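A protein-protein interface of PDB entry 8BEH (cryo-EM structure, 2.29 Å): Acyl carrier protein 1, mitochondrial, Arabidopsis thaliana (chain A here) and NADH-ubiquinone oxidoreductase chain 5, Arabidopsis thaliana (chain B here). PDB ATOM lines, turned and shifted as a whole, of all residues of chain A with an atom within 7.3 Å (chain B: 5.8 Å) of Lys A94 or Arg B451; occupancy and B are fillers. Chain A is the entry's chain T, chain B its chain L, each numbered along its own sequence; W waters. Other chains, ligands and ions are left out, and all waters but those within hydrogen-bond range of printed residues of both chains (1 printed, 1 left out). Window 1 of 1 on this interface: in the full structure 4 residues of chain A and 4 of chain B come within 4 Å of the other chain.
The side-chain carboxylate (OE1) of Glu B362 is in salt-bridge range of the side-chain amino group (NZ) of Lys A94, at 2.9 Å. The side-chain amino group of Lys A94 lies within salt-bridge range of the side-chain carboxylate of Asp B452, at 2.9 Å.
O of His A118 lies close to OG of Ser A121 (3.4 Å).
Among the printed residues, pairs that only touch across the chains: Glu A91 with Phe B449, Phe A93 with Arg B451, Lys A94 with Phe B449, Lys A94 with Arg B451 and Ser A121 with Arg B451.
Of the printed residues of chain B, Glu A91 touches Phe B449 (3.6 Å). Of the printed residues of chain B, Phe A93 touches Arg B451 (3.7 Å). Lys A94 touches just these residues of chain B: Glu B362, Phe B449, Arg B451 and Asp B452. Of the printed residues of chain A, Glu B362 touches Lys A94. Arg B451 touches just these residues of chain A: Phe A93 (3.7 Å), Lys A94 (3.7 Å) and Ser A121 (3.7 Å). Of the printed residues of chain A, Asp B452 touches Lys A94 (2.9 Å). The nearest residue of chain B that does not touch Lys A94 is Met B359 (4.8 Å). The nearest residue of chain A that does not touch Arg B451 is Met A120 (4.2 Å). The nearest printed residue of chain B that does not touch Phe A93 is Phe B449 (5.8 Å).
Of the 10 printed residues of chain B, 4 touch a printed residue of chain A. Along chain A the printed residues that touch a printed residue of chain B span positions 91 to 121.
Water W1 lies within hydrogen-bond range of the backbone NH (N) of Arg B451, the backbone NH (N) of Gly B450, the backbone carbonyl oxygen (O) of Glu A92 and the backbone carbonyl oxygen (O) of Glu A91.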
ATOM      1  N   ARG A  49      12.670   0.267  20.902  1.00  0.00           N
ATOM      2  CA  ARG A  49      12.419   1.581  21.517  1.00  0.00           C
ATOM      3  C   ARG A  49      11.185   1.563  22.462  1.00  0.00           C
ATOM      4  O   ARG A  49      11.184   2.331  23.401  1.00  0.00           O
ATOM      5  CB  ARG A  49      12.339   2.665  20.430  1.00  0.00           C
ATOM      6  CG  ARG A  49      13.508   2.827  19.483  1.00  0.00           C
ATOM      7  CD  ARG A  49      13.165   4.190  18.936  1.00  0.00           C
ATOM      8  NE  ARG A  49      12.806   4.308  17.538  1.00  0.00           N
ATOM      9  CZ  ARG A  49      12.132   5.325  17.031  1.00  0.00           C
ATOM     10  NH1 ARG A  49      11.682   6.289  17.814  1.00  0.00           N
ATOM     11  NH2 ARG A  49      11.861   5.352  15.741  1.00  0.00           N
ATOM     12  N   ALA A  88       4.634   8.553  27.433  1.00  0.00           N
ATOM     13  CA  ALA A  88       6.057   8.494  27.110  1.00  0.00           C
ATOM     14  C   ALA A  88       6.292   7.875  25.735  1.00  0.00           C
ATOM     15  O   ALA A  88       7.161   8.330  24.987  1.00  0.00           O
ATOM     16  CB  ALA A  88       6.810   7.719  28.186  1.00  0.00           C
ATOM     17  N   ILE A  89       5.530   6.837  25.389  1.00  0.00           N
ATOM     18  CA  ILE A  89       5.615   6.251  24.050  1.00  0.00           C
ATOM     19  C   ILE A  89       5.192   7.273  22.998  1.00  0.00           C
ATOM     20  O   ILE A  89       5.812   7.394  21.928  1.00  0.00           O
ATOM     21  CB  ILE A  89       4.763   4.969  23.979  1.00  0.00           C
ATOM     22  CG1 ILE A  89       5.439   3.833  24.746  1.00  0.00           C
ATOM     23  CG2 ILE A  89       4.508   4.556  22.536  1.00  0.00           C
ATOM     24  CD1 ILE A  89       4.481   2.755  25.219  1.00  0.00           C
ATOM     25  N   GLU A  90       4.122   8.018  23.292  1.00  0.00           N
ATOM     26  CA  GLU A  90       3.664   9.101  22.428  1.00  0.00           C
ATOM     27  C   GLU A  90       4.791  10.081  22.135  1.00  0.00           C
ATOM     28  O   GLU A  90       5.039  10.438  20.980  1.00  0.00           O
ATOM     29  CB  GLU A  90       2.501   9.834  23.102  1.00  0.00           C
ATOM     30  CG  GLU A  90       1.142   9.184  22.976  1.00  0.00           C
ATOM     31  CD  GLU A  90       0.469   9.527  21.674  1.00  0.00           C
ATOM     32  OE1 GLU A  90       0.968   9.081  20.625  1.00  0.00           O
ATOM     33  OE2 GLU A  90      -0.558  10.236  21.694  1.00  0.00           O
ATOM     34  N   GLU A  91       5.616  10.468  23.124  1.00  0.00           N
ATOM     35  CA  GLU A  91       6.672  11.480  22.940  1.00  0.00           C
ATOM     36  C   GLU A  91       7.802  10.785  22.211  1.00  0.00           C
ATOM     37  O   GLU A  91       8.430  11.391  21.376  1.00  0.00           O
ATOM     38  CB  GLU A  91       7.182  12.084  24.261  1.00  0.00           C
ATOM     39  CG  GLU A  91       6.267  13.101  24.899  1.00  0.00           C
ATOM     40  CD  GLU A  91       6.981  14.003  25.896  1.00  0.00           C
ATOM     41  OE1 GLU A  91       6.304  14.768  26.603  1.00  0.00           O
ATOM     42  OE2 GLU A  91       8.225  13.944  25.949  1.00  0.00           O
ATOM     43  N   GLU A  92       7.966   9.528  22.512  1.00  0.00           N
ATOM     44  CA  GLU A  92       9.120   8.861  21.931  1.00  0.00           C
ATOM     45  C   GLU A  92       8.981   8.725  20.418  1.00  0.00           C
ATOM     46  O   GLU A  92       9.973   8.839  19.691  1.00  0.00           O
ATOM     47  CB  GLU A  92       9.317   7.495  22.587  1.00  0.00           C
ATOM     48  CG  GLU A  92      10.164   6.547  21.780  1.00  0.00           C
ATOM     49  CD  GLU A  92      11.622   6.936  21.827  1.00  0.00           C
ATOM     50  OE1 GLU A  92      11.984   7.808  22.645  1.00  0.00           O
ATOM     51  OE2 GLU A  92      12.412   6.392  21.041  1.00  0.00           O
ATOM     52  N   PHE A  93       7.768   8.529  19.869  1.00  0.00           N
ATOM     53  CA  PHE A  93       7.607   8.353  18.402  1.00  0.00           C
ATOM     54  C   PHE A  93       6.966   9.608  17.780  1.00  0.00           C
ATOM     55  O   PHE A  93       6.753   9.550  16.577  1.00  0.00           O
ATOM     56  CB  PHE A  93       6.853   7.038  18.067  1.00  0.00           C
ATOM     57  CG  PHE A  93       7.608   5.769  18.359  1.00  0.00           C
ATOM     58  CD1 PHE A  93       8.492   5.240  17.435  1.00  0.00           C
ATOM     59  CD2 PHE A  93       7.434   5.098  19.558  1.00  0.00           C
ATOM     60  CE1 PHE A  93       9.178   4.068  17.699  1.00  0.00           C
ATOM     61  CE2 PHE A  93       8.128   3.933  19.827  1.00  0.00           C
ATOM     62  CZ  PHE A  93       8.997   3.419  18.894  1.00  0.00           C
ATOM     63  N   LYS A  94       6.679  10.682  18.558  1.00  0.00           N
ATOM     64  CA  LYS A  94       5.957  11.889  18.037  1.00  0.00           C
ATOM     65  C   LYS A  94       4.590  11.482  17.451  1.00  0.00           C
ATOM     66  O   LYS A  94       4.301  11.839  16.339  1.00  0.00           O
ATOM     67  CB  LYS A  94       6.785  12.851  17.161  1.00  0.00           C
ATOM     68  CG  LYS A  94       6.272  14.279  17.167  1.00  0.00           C
ATOM     69  CD  LYS A  94       6.841  15.223  16.138  1.00  0.00           C
ATOM     70  CE  LYS A  94       6.222  16.603  16.278  1.00  0.00           C
ATOM     71  NZ  LYS A  94       6.765  17.600  15.328  1.00  0.00           N
ATOM     72  N   LEU A  95       3.726  10.918  18.273  1.00  0.00           N
ATOM     73  CA  LEU A  95       2.390  10.596  17.801  1.00  0.00           C
ATOM     74  C   LEU A  95       1.361  11.282  18.686  1.00  0.00           C
ATOM     75  O   LEU A  95       1.648  11.684  19.815  1.00  0.00           O
ATOM     76  CB  LEU A  95       2.134   9.084  17.775  1.00  0.00           C
ATOM     77  CG  LEU A  95       3.231   8.192  17.202  1.00  0.00           C
ATOM     78  CD1 LEU A  95       3.043   6.749  17.649  1.00  0.00           C
ATOM     79  CD2 LEU A  95       3.300   8.306  15.694  1.00  0.00           C
ATOM     80  N   GLU A  96       0.155  11.428  18.152  1.00  0.00           N
ATOM     81  CA  GLU A  96      -0.981  11.953  18.904  1.00  0.00           C
ATOM     82  C   GLU A  96      -2.077  10.895  18.847  1.00  0.00           C
ATOM     83  O   GLU A  96      -2.897  10.891  17.926  1.00  0.00           O
ATOM     84  CB  GLU A  96      -1.455  13.293  18.348  1.00  0.00           C
ATOM     85  CG  GLU A  96      -2.425  14.027  19.258  1.00  0.00           C
ATOM     86  CD  GLU A  96      -2.259  15.541  19.210  1.00  0.00           C
ATOM     87  OE1 GLU A  96      -1.110  16.016  19.242  1.00  0.00           O
ATOM     88  OE2 GLU A  96      -3.279  16.255  19.153  1.00  0.00           O
ATOM     89  N   ILE A  97      -2.074   9.993  19.816  1.00  0.00           N
ATOM     90  CA  ILE A  97      -3.080   8.931  19.872  1.00  0.00           C
ATOM     91  C   ILE A  97      -4.390   9.518  20.392  1.00  0.00           C
ATOM     92  O   ILE A  97      -4.374  10.267  21.379  1.00  0.00           O
ATOM     93  CB  ILE A  97      -2.601   7.786  20.756  1.00  0.00           C
ATOM     94  CG1 ILE A  97      -1.357   7.146  20.151  1.00  0.00           C
ATOM     95  CG2 ILE A  97      -3.694   6.737  20.907  1.00  0.00           C
ATOM     96  CD1 ILE A  97      -0.582   6.275  21.103  1.00  0.00           C
ATOM     97  N   HIS A 118       1.085   2.441  12.791  1.00  0.00           N
ATOM     98  CA  HIS A 118       0.859   3.846  12.494  1.00  0.00           C
ATOM     99  C   HIS A 118       1.797   4.281  11.375  1.00  0.00           C
ATOM    100  O   HIS A 118       3.014   4.107  11.490  1.00  0.00           O
ATOM    101  CB  HIS A 118       1.062   4.726  13.722  1.00  0.00           C
ATOM    102  CG  HIS A 118       0.317   6.020  13.648  1.00  0.00           C
ATOM    103  ND1 HIS A 118      -0.802   6.183  12.865  1.00  0.00           N
ATOM    104  CD2 HIS A 118       0.554   7.224  14.215  1.00  0.00           C
ATOM    105  CE1 HIS A 118      -1.239   7.424  12.972  1.00  0.00           C
ATOM    106  NE2 HIS A 118      -0.431   8.078  13.783  1.00  0.00           N
ATOM    107  N   MET A 120       2.695   7.245  10.456  1.00  0.00           N
ATOM    108  CA  MET A 120       3.475   8.438  10.736  1.00  0.00           C
ATOM    109  C   MET A 120       4.484   8.237  11.857  1.00  0.00           C
ATOM    110  O   MET A 120       5.121   9.205  12.277  1.00  0.00           O
ATOM    111  CB  MET A 120       2.554   9.610  11.070  1.00  0.00           C
ATOM    112  CG  MET A 120       1.867  10.202   9.858  1.00  0.00           C
ATOM    113  SD  MET A 120       2.932  11.261   8.867  1.00  0.00           S
ATOM    114  CE  MET A 120       3.994  11.987  10.105  1.00  0.00           C
ATOM    115  N   SER A 121       4.694   7.020  12.346  1.00  0.00           N
ATOM    116  CA  SER A 121       5.716   6.783  13.408  1.00  0.00           C
ATOM    117  C   SER A 121       7.151   6.927  12.877  1.00  0.00           C
ATOM    118  O   SER A 121       8.023   7.354  13.648  1.00  0.00           O
ATOM    119  CB  SER A 121       5.506   5.448  14.054  1.00  0.00           C
ATOM    120  OG  SER A 121       4.170   5.301  14.505  1.00  0.00           O
ATOM    121  N   MET B 359      12.583  21.589  10.928  1.00  0.00           N
ATOM    122  CA  MET B 359      11.988  20.893  12.059  1.00  0.00           C
ATOM    123  C   MET B 359      10.772  20.064  11.658  1.00  0.00           C
ATOM    124  O   MET B 359       9.882  19.835  12.480  1.00  0.00           O
ATOM    125  CB  MET B 359      11.614  21.897  13.147  1.00  0.00           C
ATOM    126  CG  MET B 359      12.795  22.478  13.899  1.00  0.00           C
ATOM    127  SD  MET B 359      14.046  21.254  14.299  1.00  0.00           S
ATOM    128  CE  MET B 359      13.452  20.721  15.901  1.00  0.00           C
ATOM    129  N   SER B 360      10.749  19.611  10.408  1.00  0.00           N
ATOM    130  CA  SER B 360       9.645  18.772   9.832  1.00  0.00           C
ATOM    131  C   SER B 360       8.296  19.446   9.989  1.00  0.00           C
ATOM    132  O   SER B 360       7.368  18.767  10.419  1.00  0.00           O
ATOM    133  CB  SER B 360       9.703  17.402  10.427  1.00  0.00           C
ATOM    134  OG  SER B 360      11.030  16.954  10.579  1.00  0.00           O
ATOM    135  N   GLU B 362       7.292  21.615  12.252  1.00  0.00           N
ATOM    136  CA  GLU B 362       6.893  22.033  13.586  1.00  0.00           C
ATOM    137  C   GLU B 362       6.921  23.555  13.652  1.00  0.00           C
ATOM    138  O   GLU B 362       7.906  24.185  13.260  1.00  0.00           O
ATOM    139  CB  GLU B 362       7.815  21.428  14.646  1.00  0.00           C
ATOM    140  CG  GLU B 362       7.468  21.823  16.070  1.00  0.00           C
ATOM    141  CD  GLU B 362       6.087  21.346  16.489  1.00  0.00           C
ATOM    142  OE1 GLU B 362       5.871  20.118  16.563  1.00  0.00           O
ATOM    143  OE2 GLU B 362       5.214  22.198  16.743  1.00  0.00           O
ATOM    144  N   PHE B 449      11.149  17.138  19.990  1.00  0.00           N
ATOM    145  CA  PHE B 449      11.026  15.681  19.871  1.00  0.00           C
ATOM    146  C   PHE B 449      12.353  15.183  19.285  1.00  0.00           C
ATOM    147  O   PHE B 449      12.894  15.864  18.429  1.00  0.00           O
ATOM    148  CB  PHE B 449       9.794  15.422  18.986  1.00  0.00           C
ATOM    149  CG  PHE B 449       8.446  15.702  19.601  1.00  0.00           C
ATOM    150  CD1 PHE B 449       7.795  16.903  19.381  1.00  0.00           C
ATOM    151  CD2 PHE B 449       7.793  14.740  20.354  1.00  0.00           C
ATOM    152  CE1 PHE B 449       6.543  17.153  19.919  1.00  0.00           C
ATOM    153  CE2 PHE B 449       6.542  14.989  20.896  1.00  0.00           C
ATOM    154  CZ  PHE B 449       5.916  16.194  20.677  1.00  0.00           C
ATOM    155  N   GLY B 450      12.886  14.077  19.764  1.00  0.00           N
ATOM    156  CA  GLY B 450      14.089  13.497  19.176  1.00  0.00           C
ATOM    157  C   GLY B 450      13.975  13.237  17.702  1.00  0.00           C
ATOM    158  O   GLY B 450      14.950  13.526  16.998  1.00  0.00           O
ATOM    159  N   ARG B 451      12.811  12.788  17.226  1.00  0.00           N
ATOM    160  CA  ARG B 451      12.683  12.451  15.782  1.00  0.00           C
ATOM    161  C   ARG B 451      12.866  13.730  14.948  1.00  0.00           C
ATOM    162  O   ARG B 451      13.311  13.609  13.792  1.00  0.00           O
ATOM    163  CB  ARG B 451      11.358  11.735  15.486  1.00  0.00           C
ATOM    164  CG  ARG B 451      11.145  11.329  14.035  1.00  0.00           C
ATOM    165  CD  ARG B 451       9.867  10.558  13.755  1.00  0.00           C
ATOM    166  NE  ARG B 451       8.646  11.318  13.981  1.00  0.00           N
ATOM    167  CZ  ARG B 451       8.108  12.157  13.103  1.00  0.00           C
ATOM    168  NH1 ARG B 451       8.691  12.358  11.934  1.00  0.00           N
ATOM    169  NH2 ARG B 451       6.995  12.802  13.403  1.00  0.00           N
ATOM    170  N   ASP B 452      12.551  14.903  15.513  1.00  0.00           N
ATOM    171  CA  ASP B 452      12.743  16.172  14.769  1.00  0.00           C
ATOM    172  C   ASP B 452      14.242  16.541  14.700  1.00  0.00           C
ATOM    173  O   ASP B 452      14.686  16.795  13.632  1.00  0.00           O
ATOM    174  CB  ASP B 452      11.808  17.278  15.299  1.00  0.00           C
ATOM    175  CG  ASP B 452      10.334  17.057  15.040  1.00  0.00           C
ATOM    176  OD1 ASP B 452       9.986  16.608  13.940  1.00  0.00           O
ATOM    177  OD2 ASP B 452       9.556  17.351  15.936  1.00  0.00           O
ATOM    178  N   ILE B 453      14.975  16.396  15.792  1.00  0.00           N
ATOM    179  CA  ILE B 453      16.420  16.782  15.909  1.00  0.00           C
ATOM    180  C   ILE B 453      17.261  15.923  14.988  1.00  0.00           C
ATOM    181  O   ILE B 453      18.067  16.460  14.278  1.00  0.00           O
ATOM    182  CB  ILE B 453      16.764  16.603  17.407  1.00  0.00           C
ATOM    183  CG1 ILE B 453      16.295  17.795  18.239  1.00  0.00           C
ATOM    184  CG2 ILE B 453      18.242  16.323  17.614  1.00  0.00           C
ATOM    185  CD1 ILE B 453      16.653  19.122  17.628  1.00  0.00           C
ATOM    186  N   SER B 454      16.884  14.673  14.841  1.00  0.00           N
ATOM    187  CA  SER B 454      17.627  13.643  14.119  1.00  0.00           C
ATOM    188  C   SER B 454      17.367  13.677  12.612  1.00  0.00           C
ATOM    189  O   SER B 454      18.047  13.015  11.927  1.00  0.00           O
ATOM    190  CB  SER B 454      17.233  12.361  14.812  1.00  0.00           C
ATOM    191  OG  SER B 454      18.065  12.133  15.924  1.00  0.00           O
ATOM    192  N   ARG B 455      16.546  14.595  12.157  1.00  0.00           N
ATOM    193  CA  ARG B 455      16.205  14.754  10.738  1.00  0.00           C
ATOM    194  C   ARG B 455      16.426  16.228  10.313  1.00  0.00           C
ATOM    195  O   ARG B 455      15.964  16.549   9.235  1.00  0.00           O
ATOM    196  CB  ARG B 455      14.765  14.299  10.559  1.00  0.00           C
ATOM    197  CG  ARG B 455      14.490  12.828  10.806  1.00  0.00           C
ATOM    198  CD  ARG B 455      13.023  12.566  10.543  1.00  0.00           C
ATOM    199  NE  ARG B 455      12.794  11.920   9.264  1.00  0.00           N
ATOM    200  CZ  ARG B 455      12.394  10.660   9.116  1.00  0.00           C
ATOM    201  NH1 ARG B 455      12.152   9.908  10.177  1.00  0.00           N
ATOM    202  NH2 ARG B 455      12.222  10.162   7.905  1.00  0.00           N
HETATM  203  O   HOH W   1      10.648  11.953  18.995  1.00  0.00           O
